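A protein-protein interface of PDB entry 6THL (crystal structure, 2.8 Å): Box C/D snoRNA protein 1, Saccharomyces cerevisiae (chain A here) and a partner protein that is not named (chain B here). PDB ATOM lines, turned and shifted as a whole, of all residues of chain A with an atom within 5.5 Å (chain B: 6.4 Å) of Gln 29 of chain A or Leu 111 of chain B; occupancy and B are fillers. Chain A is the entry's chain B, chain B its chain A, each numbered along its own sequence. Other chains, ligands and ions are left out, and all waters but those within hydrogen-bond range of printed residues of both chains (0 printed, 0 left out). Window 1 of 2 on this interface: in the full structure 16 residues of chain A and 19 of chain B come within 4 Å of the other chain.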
ATOM      1  N   MET A  24     -10.944  -9.794  13.327  1.00  0.00           N
ATOM      2  CA  MET A  24      -9.637  -9.403  13.813  1.00  0.00           C
ATOM      3  C   MET A  24      -9.799  -8.860  15.213  1.00  0.00           C
ATOM      4  O   MET A  24     -10.770  -8.188  15.500  1.00  0.00           O
ATOM      5  CB  MET A  24      -8.977  -8.377  12.893  1.00  0.00           C
ATOM      6  CG  MET A  24      -8.667  -8.884  11.496  1.00  0.00           C
ATOM      7  SD  MET A  24      -7.381 -10.145  11.462  1.00  0.00           S
ATOM      8  CE  MET A  24      -7.889 -10.958   9.957  1.00  0.00           C
ATOM      9  N   GLN A  25      -8.854  -9.204  16.082  1.00  0.00           N
ATOM     10  CA  GLN A  25      -8.905  -8.813  17.470  1.00  0.00           C
ATOM     11  C   GLN A  25      -9.174  -7.305  17.562  1.00  0.00           C
ATOM     12  O   GLN A  25     -10.081  -6.873  18.282  1.00  0.00           O
ATOM     13  CB  GLN A  25      -7.599  -9.218  18.173  1.00  0.00           C
ATOM     14  CG  GLN A  25      -7.632  -8.953  19.663  1.00  0.00           C
ATOM     15  CD  GLN A  25      -6.757  -9.874  20.484  1.00  0.00           C
ATOM     16  OE1 GLN A  25      -7.062 -11.053  20.628  1.00  0.00           O
ATOM     17  NE2 GLN A  25      -5.687  -9.331  21.067  1.00  0.00           N
ATOM     18  N   ARG A  26      -8.430  -6.514  16.784  1.00  0.00           N
ATOM     19  CA  ARG A  26      -8.514  -5.061  16.843  1.00  0.00           C
ATOM     20  C   ARG A  26      -9.926  -4.626  16.526  1.00  0.00           C
ATOM     21  O   ARG A  26     -10.460  -3.692  17.147  1.00  0.00           O
ATOM     22  CB  ARG A  26      -7.537  -4.357  15.892  1.00  0.00           C
ATOM     23  CG  ARG A  26      -7.605  -2.827  15.965  1.00  0.00           C
ATOM     24  CD  ARG A  26      -6.359  -2.094  15.442  1.00  0.00           C
ATOM     25  NE  ARG A  26      -6.450  -0.676  15.789  1.00  0.00           N
ATOM     26  CZ  ARG A  26      -5.791  -0.063  16.769  1.00  0.00           C
ATOM     27  NH1 ARG A  26      -4.870  -0.695  17.464  1.00  0.00           N
ATOM     28  NH2 ARG A  26      -6.018   1.238  17.004  1.00  0.00           N
ATOM     29  N   SER A  27     -10.540  -5.306  15.574  1.00  0.00           N
ATOM     30  CA  SER A  27     -11.876  -4.942  15.177  1.00  0.00           C
ATOM     31  C   SER A  27     -12.783  -5.056  16.383  1.00  0.00           C
ATOM     32  O   SER A  27     -13.606  -4.197  16.645  1.00  0.00           O
ATOM     33  CB  SER A  27     -12.352  -5.826  14.029  1.00  0.00           C
ATOM     34  OG  SER A  27     -13.708  -5.623  13.792  1.00  0.00           O
ATOM     35  N   SER A  28     -12.579  -6.081  17.178  1.00  0.00           N
ATOM     36  CA  SER A  28     -13.389  -6.233  18.364  1.00  0.00           C
ATOM     37  C   SER A  28     -12.868  -5.366  19.465  1.00  0.00           C
ATOM     38  O   SER A  28     -13.507  -5.307  20.505  1.00  0.00           O
ATOM     39  CB  SER A  28     -13.449  -7.695  18.837  1.00  0.00           C
ATOM     40  OG  SER A  28     -14.027  -8.548  17.844  1.00  0.00           O
ATOM     41  N   GLN A  29     -11.723  -4.705  19.315  1.00  0.00           N
ATOM     42  CA  GLN A  29     -11.358  -3.747  20.388  1.00  0.00           C
ATOM     43  C   GLN A  29     -11.653  -2.298  20.050  1.00  0.00           C
ATOM     44  O   GLN A  29     -11.323  -1.430  20.834  1.00  0.00           O
ATOM     45  CB  GLN A  29      -9.942  -3.950  20.979  1.00  0.00           C
ATOM     46  CG  GLN A  29      -8.920  -4.518  20.020  1.00  0.00           C
ATOM     47  CD  GLN A  29      -7.512  -4.625  20.570  1.00  0.00           C
ATOM     48  OE1 GLN A  29      -6.727  -5.368  20.037  1.00  0.00           O
ATOM     49  NE2 GLN A  29      -7.192  -3.887  21.610  1.00  0.00           N
ATOM     50  N   ASN A  30     -12.336  -2.066  18.928  1.00  0.00           N
ATOM     51  CA  ASN A  30     -12.865  -0.740  18.563  1.00  0.00           C
ATOM     52  C   ASN A  30     -14.290  -0.509  19.099  1.00  0.00           C
ATOM     53  O   ASN A  30     -15.206  -1.246  18.751  1.00  0.00           O
ATOM     54  CB  ASN A  30     -12.869  -0.568  17.027  1.00  0.00           C
ATOM     55  CG  ASN A  30     -12.964   0.898  16.592  1.00  0.00           C
ATOM     56  OD1 ASN A  30     -13.229   1.815  17.374  1.00  0.00           O
ATOM     57  ND2 ASN A  30     -12.741   1.116  15.333  1.00  0.00           N
ATOM     58  N   ARG A  31     -14.473   0.507  19.941  1.00  0.00           N
ATOM     59  CA  ARG A  31     -15.829   0.918  20.355  1.00  0.00           C
ATOM     60  C   ARG A  31     -16.174   2.372  19.929  1.00  0.00           C
ATOM     61  O   ARG A  31     -17.220   2.911  20.310  1.00  0.00           O
ATOM     62  CB  ARG A  31     -16.041   0.687  21.877  1.00  0.00           C
ATOM     63  CG  ARG A  31     -16.085  -0.782  22.293  1.00  0.00           C
ATOM     64  CD  ARG A  31     -16.600  -1.042  23.723  1.00  0.00           C
ATOM     65  NE  ARG A  31     -16.076  -2.317  24.244  1.00  0.00           N
ATOM     66  CZ  ARG A  31     -16.134  -2.734  25.514  1.00  0.00           C
ATOM     67  NH1 ARG A  31     -16.725  -2.019  26.470  1.00  0.00           N
ATOM     68  NH2 ARG A  31     -15.577  -3.892  25.850  1.00  0.00           N
ATOM     69  N   SER A  44     -12.418   5.253  20.896  1.00  0.00           N
ATOM     70  CA  SER A  44     -11.505   4.386  21.563  1.00  0.00           C
ATOM     71  C   SER A  44     -10.102   4.855  21.113  1.00  0.00           C
ATOM     72  O   SER A  44      -9.877   5.101  19.918  1.00  0.00           O
ATOM     73  CB  SER A  44     -11.812   2.935  21.175  1.00  0.00           C
ATOM     74  OG  SER A  44     -13.215   2.780  20.960  1.00  0.00           O
ATOM     75  N   VAL A  65      -6.290   0.291  26.239  1.00  0.00           N
ATOM     76  CA  VAL A  65      -7.288   0.809  25.327  1.00  0.00           C
ATOM     77  C   VAL A  65      -8.435   1.434  26.097  1.00  0.00           C
ATOM     78  O   VAL A  65      -9.085   0.746  26.867  1.00  0.00           O
ATOM     79  CB  VAL A  65      -7.825  -0.330  24.467  1.00  0.00           C
ATOM     80  CG1 VAL A  65      -8.887   0.154  23.495  1.00  0.00           C
ATOM     81  CG2 VAL A  65      -6.662  -0.938  23.717  1.00  0.00           C
ATOM     82  N   HIS A  67     -12.040   3.717  26.067  1.00  0.00           N
ATOM     83  CA  HIS A  67     -13.194   3.788  25.207  1.00  0.00           C
ATOM     84  C   HIS A  67     -13.976   5.063  25.489  1.00  0.00           C
ATOM     85  O   HIS A  67     -13.805   5.679  26.526  1.00  0.00           O
ATOM     86  CB  HIS A  67     -14.108   2.603  25.500  1.00  0.00           C
ATOM     87  CG  HIS A  67     -13.574   1.277  25.062  1.00  0.00           C
ATOM     88  ND1 HIS A  67     -13.397   0.945  23.738  1.00  0.00           N
ATOM     89  CD2 HIS A  67     -13.274   0.168  25.771  1.00  0.00           C
ATOM     90  CE1 HIS A  67     -12.968  -0.298  23.648  1.00  0.00           C
ATOM     91  NE2 HIS A  67     -12.881  -0.790  24.871  1.00  0.00           N
ATOM     92  N   PHE A 163      -8.846   3.244  14.702  1.00  0.00           N
ATOM     93  CA  PHE A 163      -8.915   4.166  15.815  1.00  0.00           C
ATOM     94  C   PHE A 163      -7.487   4.441  16.239  1.00  0.00           C
ATOM     95  O   PHE A 163      -6.625   3.541  16.202  1.00  0.00           O
ATOM     96  CB  PHE A 163      -9.776   3.639  17.022  1.00  0.00           C
ATOM     97  CG  PHE A 163      -9.176   2.451  17.784  1.00  0.00           C
ATOM     98  CD1 PHE A 163      -8.477   2.637  18.937  1.00  0.00           C
ATOM     99  CD2 PHE A 163      -9.352   1.152  17.340  1.00  0.00           C
ATOM    100  CE1 PHE A 163      -7.942   1.561  19.627  1.00  0.00           C
ATOM    101  CE2 PHE A 163      -8.815   0.073  18.018  1.00  0.00           C
ATOM    102  CZ  PHE A 163      -8.121   0.276  19.171  1.00  0.00           C
ATOM    103  N   LYS B  14      -4.448 -12.518  20.018  1.00  0.00           N
ATOM    104  CA  LYS B  14      -3.119 -12.210  20.489  1.00  0.00           C
ATOM    105  C   LYS B  14      -3.248 -12.080  21.991  1.00  0.00           C
ATOM    106  O   LYS B  14      -3.929 -11.166  22.465  1.00  0.00           O
ATOM    107  CB  LYS B  14      -2.649 -10.869  19.880  1.00  0.00           C
ATOM    108  CG  LYS B  14      -1.178 -10.477  20.116  1.00  0.00           C
ATOM    109  CD  LYS B  14      -0.805  -9.160  19.413  1.00  0.00           C
ATOM    110  CE  LYS B  14      -0.506  -9.301  17.894  1.00  0.00           C
ATOM    111  NZ  LYS B  14      -0.852  -8.117  17.012  1.00  0.00           N
ATOM    112  N   LEU B  15      -2.638 -13.007  22.720  1.00  0.00           N
ATOM    113  CA  LEU B  15      -2.558 -12.923  24.150  1.00  0.00           C
ATOM    114  C   LEU B  15      -1.106 -12.938  24.646  1.00  0.00           C
ATOM    115  O   LEU B  15      -0.444 -13.974  24.524  1.00  0.00           O
ATOM    116  CB  LEU B  15      -3.252 -14.134  24.731  1.00  0.00           C
ATOM    117  CG  LEU B  15      -3.309 -14.096  26.282  1.00  0.00           C
ATOM    118  CD1 LEU B  15      -4.202 -12.940  26.742  1.00  0.00           C
ATOM    119  CD2 LEU B  15      -3.807 -15.412  26.849  1.00  0.00           C
ATOM    120  N   GLU B  16      -0.603 -11.845  25.189  1.00  0.00           N
ATOM    121  CA  GLU B  16       0.714 -11.851  25.772  1.00  0.00           C
ATOM    122  C   GLU B  16       0.796 -12.601  27.090  1.00  0.00           C
ATOM    123  O   GLU B  16      -0.084 -12.509  27.948  1.00  0.00           O
ATOM    124  CB  GLU B  16       1.185 -10.432  26.012  1.00  0.00           C
ATOM    125  CG  GLU B  16       1.641  -9.720  24.764  1.00  0.00           C
ATOM    126  CD  GLU B  16       1.264  -8.285  24.811  1.00  0.00           C
ATOM    127  OE1 GLU B  16       1.150  -7.794  25.937  1.00  0.00           O
ATOM    128  OE2 GLU B  16       1.038  -7.677  23.755  1.00  0.00           O
ATOM    129  N   ASN B 106      -7.207  -9.184  33.288  1.00  0.00           N
ATOM    130  CA  ASN B 106      -6.737  -7.809  33.296  1.00  0.00           C
ATOM    131  C   ASN B 106      -6.204  -7.447  31.909  1.00  0.00           C
ATOM    132  O   ASN B 106      -6.427  -6.348  31.421  1.00  0.00           O
ATOM    133  CB  ASN B 106      -5.735  -7.564  34.429  1.00  0.00           C
ATOM    134  CG  ASN B 106      -6.370  -7.699  35.812  1.00  0.00           C
ATOM    135  OD1 ASN B 106      -7.577  -7.511  35.982  1.00  0.00           O
ATOM    136  ND2 ASN B 106      -5.558  -8.050  36.809  1.00  0.00           N
ATOM    137  N   GLN B 107      -5.567  -8.399  31.246  1.00  0.00           N
ATOM    138  CA  GLN B 107      -5.129  -8.210  29.869  1.00  0.00           C
ATOM    139  C   GLN B 107      -6.276  -7.999  28.876  1.00  0.00           C
ATOM    140  O   GLN B 107      -6.192  -7.150  27.989  1.00  0.00           O
ATOM    141  CB  GLN B 107      -4.311  -9.420  29.413  1.00  0.00           C
ATOM    142  CG  GLN B 107      -3.942  -9.311  27.947  1.00  0.00           C
ATOM    143  CD  GLN B 107      -2.670 -10.040  27.567  1.00  0.00           C
ATOM    144  OE1 GLN B 107      -2.065 -10.757  28.371  1.00  0.00           O
ATOM    145  NE2 GLN B 107      -2.263  -9.858  26.301  1.00  0.00           N
ATOM    146  N   PHE B 108      -7.321  -8.813  28.988  1.00  0.00           N
ATOM    147  CA  PHE B 108      -8.531  -8.605  28.189  1.00  0.00           C
ATOM    148  C   PHE B 108      -9.079  -7.220  28.471  1.00  0.00           C
ATOM    149  O   PHE B 108      -9.641  -6.563  27.594  1.00  0.00           O
ATOM    150  CB  PHE B 108      -9.586  -9.658  28.523  1.00  0.00           C
ATOM    151  CG  PHE B 108      -9.549 -10.847  27.623  1.00  0.00           C
ATOM    152  CD1 PHE B 108      -8.428 -11.663  27.571  1.00  0.00           C
ATOM    153  CD2 PHE B 108     -10.640 -11.163  26.819  1.00  0.00           C
ATOM    154  CE1 PHE B 108      -8.385 -12.762  26.727  1.00  0.00           C
ATOM    155  CE2 PHE B 108     -10.597 -12.280  25.981  1.00  0.00           C
ATOM    156  CZ  PHE B 108      -9.463 -13.073  25.929  1.00  0.00           C
ATOM    157  N   LYS B 109      -8.924  -6.774  29.716  1.00  0.00           N
ATOM    158  CA  LYS B 109      -9.372  -5.438  30.095  1.00  0.00           C
ATOM    159  C   LYS B 109      -8.470  -4.361  29.462  1.00  0.00           C
ATOM    160  O   LYS B 109      -8.962  -3.455  28.808  1.00  0.00           O
ATOM    161  CB  LYS B 109      -9.482  -5.294  31.607  1.00  0.00           C
ATOM    162  CG  LYS B 109     -10.715  -5.969  32.198  1.00  0.00           C
ATOM    163  CD  LYS B 109     -10.753  -5.778  33.715  1.00  0.00           C
ATOM    164  CE  LYS B 109     -11.541  -6.827  34.483  1.00  0.00           C
ATOM    165  NZ  LYS B 109     -11.060  -6.905  35.907  1.00  0.00           N
ATOM    166  N   LYS B 110      -7.162  -4.500  29.580  1.00  0.00           N
ATOM    167  CA  LYS B 110      -6.265  -3.535  28.944  1.00  0.00           C
ATOM    168  C   LYS B 110      -6.353  -3.551  27.368  1.00  0.00           C
ATOM    169  O   LYS B 110      -6.045  -2.562  26.690  1.00  0.00           O
ATOM    170  CB  LYS B 110      -4.841  -3.678  29.526  1.00  0.00           C
ATOM    171  CG  LYS B 110      -4.722  -3.297  31.020  1.00  0.00           C
ATOM    172  CD  LYS B 110      -3.590  -4.087  31.683  1.00  0.00           C
ATOM    173  CE  LYS B 110      -3.506  -3.874  33.214  1.00  0.00           C
ATOM    174  NZ  LYS B 110      -2.153  -4.097  33.861  1.00  0.00           N
ATOM    175  N   LEU B 111      -6.865  -4.629  26.783  1.00  0.00           N
ATOM    176  CA  LEU B 111      -7.167  -4.610  25.346  1.00  0.00           C
ATOM    177  C   LEU B 111      -8.531  -3.980  25.081  1.00  0.00           C
ATOM    178  O   LEU B 111      -8.928  -3.843  23.937  1.00  0.00           O
ATOM    179  CB  LEU B 111      -7.086  -6.032  24.745  1.00  0.00           C
ATOM    180  CG  LEU B 111      -5.736  -6.786  24.811  1.00  0.00           C
ATOM    181  CD1 LEU B 111      -5.755  -8.132  24.068  1.00  0.00           C
ATOM    182  CD2 LEU B 111      -4.572  -5.918  24.317  1.00  0.00           C
ATOM    183  N   GLY B 112      -9.277  -3.627  26.122  1.00  0.00           N
ATOM    184  CA  GLY B 112     -10.634  -3.137  25.927  1.00  0.00           C
ATOM    185  C   GLY B 112     -11.595  -4.210  25.403  1.00  0.00           C
ATOM    186  O   GLY B 112     -12.625  -3.886  24.744  1.00  0.00           O
ATOM    187  N   LEU B 113     -11.299  -5.488  25.689  1.00  0.00           N
ATOM    188  CA  LEU B 113     -12.213  -6.544  25.278  1.00  0.00           C
ATOM    189  C   LEU B 113     -13.292  -6.754  26.312  1.00  0.00           C
ATOM    190  O   LEU B 113     -14.350  -7.238  25.974  1.00  0.00           O
ATOM    191  CB  LEU B 113     -11.501  -7.860  24.948  1.00  0.00           C
ATOM    192  CG  LEU B 113     -10.560  -7.810  23.729  1.00  0.00           C
ATOM    193  CD1 LEU B 113      -9.609  -9.005  23.729  1.00  0.00           C
ATOM    194  CD2 LEU B 113     -11.311  -7.711  22.391  1.00  0.00           C
ATOM    195  N   LEU B 114     -13.049  -6.405  27.564  1.00  0.00           N
ATOM    196  CA  LEU B 114     -14.062  -6.611  28.575  1.00  0.00           C
ATOM    197  C   LEU B 114     -13.978  -5.485  29.582  1.00  0.00           C
ATOM    198  O   LEU B 114     -12.900  -4.980  29.834  1.00  0.00           O
ATOM    199  CB  LEU B 114     -13.842  -7.955  29.256  1.00  0.00           C
ATOM    200  CG  LEU B 114     -13.773  -9.243  28.412  1.00  0.00           C
ATOM    201  CD1 LEU B 114     -13.345 -10.409  29.309  1.00  0.00           C
ATOM    202  CD2 LEU B 114     -15.073  -9.568  27.687  1.00  0.00           C
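The backbone carbonyl oxygen (O) of Lys 110 of chain B is in hydrogen-bond range of the backbone NH (N) of Val 65 of chain A (2.9 Å).
The backbone carbonyl oxygen of Gly 112 of chain B lies within hydrogen-bond range of a ring nitrogen (NE2) of His 67 of chain A, at 3.1 Å.
The side-chain amide nitrogen of Gln 29 of chain A is in hydrogen-bond range of the backbone carbonyl oxygen of Leu 111 of chain B, 2.9 Å away.
O of Lys 14 of chain B sits at hydrogen-bond distance from NE2 of Gln 25 of chain A (2.9 Å).
O of Gly 112 of chain B sits at hydrogen-bond distance from NH2 of Arg 31 of chain A, at 3.2 Å.
The backbone NH of Leu 113 of chain B lies within hydrogen-bond range of the backbone carbonyl oxygen of Phe 108 of chain B (2.7 Å).
The backbone NH (N) of Arg 31 of chain A sits at hydrogen-bond distance from the side-chain hydroxyl (OG) of Ser 44 of chain A (2.8 Å).
The backbone carbonyl oxygen (O) of Phe 108 of chain B sits at hydrogen-bond distance from the backbone NH (N) of Leu 114 of chain B.
The side-chain hydroxyl (OG) of Ser 44 of chain A sits at hydrogen-bond distance from a ring nitrogen (ND1) of His 67 of chain A (3.3 Å).
Among the printed residues, pairs that only touch across the chains: Gln 25 of chain A with Leu 111 of chain B (3.2 Å), Ser 28 of chain A with Leu 113 of chain B (3.8 Å), Arg 31 of chain A with Leu 113 of chain B (3.6 Å), Arg 31 of chain A with Leu 114 of chain B (3.96 Å), Val 65 of chain A with Leu 111 of chain B (3.7 Å) and Val 65 of chain A with Gly 112 of chain B (3.96 Å).
Gln 29 of chain A touches just one residue of chain B: Leu 111 (2.9 Å).
Glu 16 of chain B touches none of the printed residues of chain A.
Of the printed residues of chain A, Lys 110 of chain B touches Val 65 (2.9 Å).
Of chain A, only Gln 25, Gln 29 and Val 65 come within 4 Å of Leu 111 of chain B.
Of the printed residues of chain A, Gly 112 of chain B touches Arg 31 (3.2 Å), Val 65 (3.96 Å) and His 67 (3.1 Å).
Of the printed residues of chain A, Leu 113 of chain B touches Ser 28 and Arg 31.
Printed residues of chain A within 4 Å of Leu 114 of chain B: Arg 31 (3.96 Å).
The nearest residue of chain B that does not touch Gln 29 of chain A is Leu 113 of chain B (4.2 Å).
The nearest residue of chain A that does not touch Leu 111 of chain B is His 67 of chain A (5.1 Å).
The nearest printed residue of chain A that does not touch Lys 14 of chain B is Gln 29 of chain A (6.8 Å).
Of the 12 printed residues of chain A, 6 touch a printed residue of chain B.
Hydrophobic or aromatic side chains of chain A within 4 Å of the printed part of chain B: Val 65 and His 67.
Of the 12 printed residues of chain B, 6 touch a printed residue of chain A.
Hydrophobic or aromatic side chains of chain B within 4 Å of the printed part of chain A: Leu 111 and Leu 113.
Along chain B the printed residues that touch a printed residue of chain A span positions 14 to 114.
Among the printed residues, 11 pairs touch across the chains.
Among the printed residues, no Asp or Glu carboxylate lies within 4 Å of a Lys or Arg side-chain nitrogen of the other chain.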
